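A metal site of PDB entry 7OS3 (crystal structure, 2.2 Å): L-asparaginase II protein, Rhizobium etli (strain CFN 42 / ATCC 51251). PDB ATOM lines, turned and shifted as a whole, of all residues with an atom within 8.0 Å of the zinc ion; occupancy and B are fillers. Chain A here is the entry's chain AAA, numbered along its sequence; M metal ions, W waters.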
ATOM      1  N   ARG A  53       2.806  19.040   7.264  1.00  0.00           N
ATOM      2  CA  ARG A  53       1.655  19.902   6.892  1.00  0.00           C
ATOM      3  C   ARG A  53       0.797  19.173   5.836  1.00  0.00           C
ATOM      4  O   ARG A  53       0.488  17.982   6.020  1.00  0.00           O
ATOM      5  CB  ARG A  53       2.224  21.253   6.441  1.00  0.00           C
ATOM      6  CG  ARG A  53       3.196  21.879   7.428  1.00  0.00           C
ATOM      7  CD  ARG A  53       2.505  22.492   8.651  1.00  0.00           C
ATOM      8  NE  ARG A  53       1.613  23.557   8.238  1.00  0.00           N
ATOM      9  CZ  ARG A  53       2.019  24.778   7.888  1.00  0.00           C
ATOM     10  NH1 ARG A  53       1.131  25.669   7.506  1.00  0.00           N
ATOM     11  NH2 ARG A  53       3.309  25.097   7.938  1.00  0.00           N
ATOM     12  N   SER A  54       0.413  19.828   4.745  1.00  0.00           N
ATOM     13  CA  SER A  54      -0.516  19.264   3.737  1.00  0.00           C
ATOM     14  C   SER A  54       0.088  18.023   3.063  1.00  0.00           C
ATOM     15  O   SER A  54      -0.705  17.251   2.490  1.00  0.00           O
ATOM     16  CB  SER A  54      -0.899  20.285   2.728  1.00  0.00           C
ATOM     17  OG  SER A  54      -1.702  21.260   3.327  1.00  0.00           O
ATOM     18  N   LYS A  57      -1.655  14.813   3.913  1.00  0.00           N
ATOM     19  CA  LYS A  57      -3.108  14.714   3.596  1.00  0.00           C
ATOM     20  C   LYS A  57      -3.478  13.315   3.099  1.00  0.00           C
ATOM     21  O   LYS A  57      -4.509  12.787   3.479  1.00  0.00           O
ATOM     22  CB  LYS A  57      -3.528  15.795   2.600  1.00  0.00           C
ATOM     23  CG  LYS A  57      -4.052  17.045   3.270  1.00  0.00           C
ATOM     24  CD  LYS A  57      -4.013  18.270   2.415  1.00  0.00           C
ATOM     25  CE  LYS A  57      -4.669  19.445   3.101  1.00  0.00           C
ATOM     26  NZ  LYS A  57      -4.328  20.731   2.447  1.00  0.00           N
ATOM     27  N   GLN A  60      -4.166  11.261   6.163  1.00  0.00           N
ATOM     28  CA  GLN A  60      -5.479  11.660   6.748  1.00  0.00           C
ATOM     29  C   GLN A  60      -6.618  11.090   5.889  1.00  0.00           C
ATOM     30  O   GLN A  60      -7.620  10.672   6.453  1.00  0.00           O
ATOM     31  CB  GLN A  60      -5.528  13.180   6.923  1.00  0.00           C
ATOM     32  CG  GLN A  60      -4.531  13.681   7.951  1.00  0.00           C
ATOM     33  CD  GLN A  60      -4.167  15.147   7.822  1.00  0.00           C
ATOM     34  OE1 GLN A  60      -3.704  15.617   6.781  1.00  0.00           O
ATOM     35  NE2 GLN A  60      -4.355  15.904   8.891  1.00  0.00           N
ATOM     36  N   ALA A  85      -6.310  17.284  -1.203  1.00  0.00           N
ATOM     37  CA  ALA A  85      -6.006  18.570  -1.882  1.00  0.00           C
ATOM     38  C   ALA A  85      -5.370  19.570  -0.917  1.00  0.00           C
ATOM     39  O   ALA A  85      -5.724  19.536   0.288  1.00  0.00           O
ATOM     40  CB  ALA A  85      -7.278  19.159  -2.447  1.00  0.00           C
ATOM     41  N   SER A  86      -4.500  20.451  -1.451  1.00  0.00           N
ATOM     42  CA  SER A  86      -4.377  21.906  -1.092  1.00  0.00           C
ATOM     43  C   SER A  86      -4.918  22.773  -2.241  1.00  0.00           C
ATOM     44  O   SER A  86      -4.125  23.371  -2.966  1.00  0.00           O
ATOM     45  CB  SER A  86      -2.943  22.262  -0.742  1.00  0.00           C
ATOM     46  OG  SER A  86      -2.505  21.607   0.466  1.00  0.00           O
ATOM     47  N   CYS A 113     -12.795  24.722   9.763  1.00  0.00           N
ATOM     48  CA  CYS A 113     -11.724  25.428   9.008  1.00  0.00           C
ATOM     49  C   CYS A 113     -12.246  26.824   8.637  1.00  0.00           C
ATOM     50  O   CYS A 113     -13.481  26.960   8.499  1.00  0.00           O
ATOM     51  CB  CYS A 113     -11.306  24.666   7.761  1.00  0.00           C
ATOM     52  SG  CYS A 113     -12.668  24.173   6.660  1.00  0.00           S
ATOM     53  N   SER A 139     -11.720  26.991   2.098  1.00  0.00           N
ATOM     54  CA  SER A 139     -10.417  26.557   2.687  1.00  0.00           C
ATOM     55  C   SER A 139      -9.734  25.585   1.732  1.00  0.00           C
ATOM     56  O   SER A 139     -10.393  24.642   1.256  1.00  0.00           O
ATOM     57  CB  SER A 139     -10.605  25.920   4.045  1.00  0.00           C
ATOM     58  OG  SER A 139      -9.429  25.204   4.421  1.00  0.00           O
ATOM     59  N   ASN A 140      -8.447  25.796   1.447  1.00  0.00           N
ATOM     60  CA  ASN A 140      -7.604  24.830   0.698  1.00  0.00           C
ATOM     61  C   ASN A 140      -7.827  23.413   1.248  1.00  0.00           C
ATOM     62  O   ASN A 140      -7.608  22.447   0.499  1.00  0.00           O
ATOM     63  CB  ASN A 140      -6.141  25.296   0.675  1.00  0.00           C
ATOM     64  CG  ASN A 140      -5.394  24.963   1.943  1.00  0.00           C
ATOM     65  OD1 ASN A 140      -5.553  25.645   2.947  1.00  0.00           O
ATOM     66  ND2 ASN A 140      -4.590  23.917   1.899  1.00  0.00           N
ATOM     67  N   CYS A 141      -8.278  23.280   2.496  1.00  0.00           N
ATOM     68  CA  CYS A 141      -8.381  21.994   3.240  1.00  0.00           C
ATOM     69  C   CYS A 141      -9.828  21.520   3.349  1.00  0.00           C
ATOM     70  O   CYS A 141     -10.061  20.526   4.089  1.00  0.00           O
ATOM     71  CB  CYS A 141      -7.817  22.145   4.641  1.00  0.00           C
ATOM     72  SG  CYS A 141      -6.017  22.344   4.598  1.00  0.00           S
ATOM     73  N   SER A 142     -10.743  22.180   2.651  1.00  0.00           N
ATOM     74  CA  SER A 142     -12.216  21.989   2.813  1.00  0.00           C
ATOM     75  C   SER A 142     -12.534  20.497   2.691  1.00  0.00           C
ATOM     76  O   SER A 142     -13.295  19.977   3.512  1.00  0.00           O
ATOM     77  CB  SER A 142     -13.002  22.819   1.800  1.00  0.00           C
ATOM     78  OG  SER A 142     -12.778  22.363   0.472  1.00  0.00           O
ATOM     79  N   LYS A 144     -10.692  17.744   3.065  1.00  0.00           N
ATOM     80  CA  LYS A 144     -10.192  16.936   4.210  1.00  0.00           C
ATOM     81  C   LYS A 144     -11.185  17.096   5.372  1.00  0.00           C
ATOM     82  O   LYS A 144     -11.521  16.088   6.034  1.00  0.00           O
ATOM     83  CB  LYS A 144      -8.790  17.356   4.644  1.00  0.00           C
ATOM     84  CG  LYS A 144      -8.362  16.780   5.983  1.00  0.00           C
ATOM     85  CD  LYS A 144      -6.967  17.191   6.395  1.00  0.00           C
ATOM     86  CE  LYS A 144      -6.722  18.674   6.202  1.00  0.00           C
ATOM     87  NZ  LYS A 144      -5.572  19.135   7.022  1.00  0.00           N
ATOM     88  N   HIS A 145     -11.648  18.335   5.598  1.00  0.00           N
ATOM     89  CA  HIS A 145     -12.572  18.668   6.703  1.00  0.00           C
ATOM     90  C   HIS A 145     -13.913  17.967   6.476  1.00  0.00           C
ATOM     91  O   HIS A 145     -14.501  17.488   7.462  1.00  0.00           O
ATOM     92  CB  HIS A 145     -12.712  20.173   6.897  1.00  0.00           C
ATOM     93  CG  HIS A 145     -11.617  20.731   7.734  1.00  0.00           C
ATOM     94  ND1 HIS A 145     -11.811  21.074   9.060  1.00  0.00           N
ATOM     95  CD2 HIS A 145     -10.321  20.962   7.451  1.00  0.00           C
ATOM     96  CE1 HIS A 145     -10.671  21.518   9.554  1.00  0.00           C
ATOM     97  NE2 HIS A 145      -9.743  21.460   8.585  1.00  0.00           N
ATOM     98  N   THR A 192      -0.835  22.401  15.573  1.00  0.00           N
ATOM     99  CA  THR A 192      -2.152  22.795  14.995  1.00  0.00           C
ATOM    100  C   THR A 192      -1.900  23.471  13.648  1.00  0.00           C
ATOM    101  O   THR A 192      -1.036  24.347  13.602  1.00  0.00           O
ATOM    102  CB  THR A 192      -2.915  23.721  15.940  1.00  0.00           C
ATOM    103  OG1 THR A 192      -3.120  23.001  17.144  1.00  0.00           O
ATOM    104  CG2 THR A 192      -4.250  24.199  15.386  1.00  0.00           C
ATOM    105  N   ASP A 193      -2.621  23.055  12.592  1.00  0.00           N
ATOM    106  CA  ASP A 193      -2.486  23.520  11.187  1.00  0.00           C
ATOM    107  C   ASP A 193      -3.253  24.838  11.038  1.00  0.00           C
ATOM    108  O   ASP A 193      -3.947  25.228  11.979  1.00  0.00           O
ATOM    109  CB  ASP A 193      -3.002  22.444  10.222  1.00  0.00           C
ATOM    110  CG  ASP A 193      -2.070  22.120   9.061  1.00  0.00           C
ATOM    111  OD1 ASP A 193      -1.295  23.032   8.630  1.00  0.00           O
ATOM    112  OD2 ASP A 193      -2.123  20.940   8.573  1.00  0.00           O
ATOM    113  N   GLY A 194      -3.121  25.503   9.874  1.00  0.00           N
ATOM    114  CA  GLY A 194      -3.838  26.753   9.523  1.00  0.00           C
ATOM    115  C   GLY A 194      -5.336  26.538   9.357  1.00  0.00           C
ATOM    116  O   GLY A 194      -6.111  27.501   9.529  1.00  0.00           O
ATOM    117  N   CYS A 195      -5.738  25.309   9.004  1.00  0.00           N
ATOM    118  CA  CYS A 195      -7.148  24.884   8.861  1.00  0.00           C
ATOM    119  C   CYS A 195      -7.713  24.401  10.201  1.00  0.00           C
ATOM    120  O   CYS A 195      -8.869  24.008  10.225  1.00  0.00           O
ATOM    121  CB  CYS A 195      -7.234  23.757   7.839  1.00  0.00           C
ATOM    122  SG  CYS A 195      -6.418  22.251   8.422  1.00  0.00           S
ATOM    123  N   ASN A 196      -6.904  24.409  11.272  1.00  0.00           N
ATOM    124  CA  ASN A 196      -7.354  24.224  12.667  1.00  0.00           C
ATOM    125  C   ASN A 196      -7.527  22.739  13.014  1.00  0.00           C
ATOM    126  O   ASN A 196      -8.336  22.435  13.909  1.00  0.00           O
ATOM    127  CB  ASN A 196      -8.649  25.004  12.885  1.00  0.00           C
ATOM    128  CG  ASN A 196      -8.962  25.279  14.331  1.00  0.00           C
ATOM    129  OD1 ASN A 196     -10.126  25.221  14.731  1.00  0.00           O
ATOM    130  ND2 ASN A 196      -7.947  25.547  15.127  1.00  0.00           N
ATOM    131  N   LEU A 197      -6.787  21.849  12.356  1.00  0.00           N
ATOM    132  CA  LEU A 197      -6.693  20.407  12.729  1.00  0.00           C
ATOM    133  C   LEU A 197      -5.325  20.131  13.329  1.00  0.00           C
ATOM    134  O   LEU A 197      -4.366  20.856  13.102  1.00  0.00           O
ATOM    135  CB  LEU A 197      -6.843  19.512  11.503  1.00  0.00           C
ATOM    136  CG  LEU A 197      -8.253  19.369  10.924  1.00  0.00           C
ATOM    137  CD1 LEU A 197      -8.179  18.840   9.497  1.00  0.00           C
ATOM    138  CD2 LEU A 197      -9.090  18.468  11.798  1.00  0.00           C
ATOM    139  N   PRO A 198      -5.184  19.007  14.043  1.00  0.00           N
ATOM    140  CA  PRO A 198      -3.863  18.522  14.415  1.00  0.00           C
ATOM    141  C   PRO A 198      -3.021  18.240  13.157  1.00  0.00           C
ATOM    142  O   PRO A 198      -3.549  17.786  12.170  1.00  0.00           O
ATOM    143  CB  PRO A 198      -4.175  17.267  15.245  1.00  0.00           C
ATOM    144  CG  PRO A 198      -5.617  17.440  15.679  1.00  0.00           C
ATOM    145  CD  PRO A 198      -6.270  18.144  14.510  1.00  0.00           C
ATOM    146  N   THR A 199      -1.721  18.525  13.201  1.00  0.00           N
ATOM    147  CA  THR A 199      -0.814  18.313  12.059  1.00  0.00           C
ATOM    148  C   THR A 199       0.441  17.667  12.626  1.00  0.00           C
ATOM    149  O   THR A 199       0.979  18.109  13.629  1.00  0.00           O
ATOM    150  CB  THR A 199      -0.625  19.630  11.272  1.00  0.00           C
ATOM    151  OG1 THR A 199      -0.087  19.343   9.980  1.00  0.00           O
ATOM    152  CG2 THR A 199       0.239  20.653  11.993  1.00  0.00           C
HETATM  153 ZN    ZN M   1      -5.087  21.386   6.645  1.00  0.00          ZN
HETATM  154  O   HOH W   1      -2.810  21.425   6.153  1.00  0.00           O
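The backbone carbonyl oxygen (O) of Cys 195 lies close to a ring nitrogen (NE2) of His 145 (3.2 Å).
SG of Cys 141 sits close to NZ of Lys 57, at 3.2 Å.
The side-chain sulfur of Cys 141 sits close to the side-chain amide nitrogen of Asn 140 (3.4 Å).
N of Cys 141 sits close to OG of Ser 139, 3.0 Å away.
The side-chain carboxylate of Asp 193 is in salt-bridge range of the guanidinium group of Arg 53 (3.0 Å).
OD2 of Asp 193 sits at hydrogen-bond distance from OG1 of Thr 199 (2.9 Å).
OD2 of Asp 193 touches the zinc ion, 3.6 Å away.
Within 4 Å of the zinc ion: Cys 141, Lys 144, Asp 193 and Cys 195.
Along chain A the residues within 4 Å of the zinc ion span positions 141 to 195.
Water W1 binds the zinc ion (2.3 Å).
The side-chain amino group (NZ) of Lys 144 binds the zinc ion (2.3 Å).
The zinc ion is bound by the side-chain sulfur (SG) of Cys 195.
SG of Cys 141 binds the zinc ion.
The zinc ion has four donor atoms within binding distance.
Water W1 bridges OD2 of Asp 193 (2.6 Å) and OG of Ser 54 (3.0 Å).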
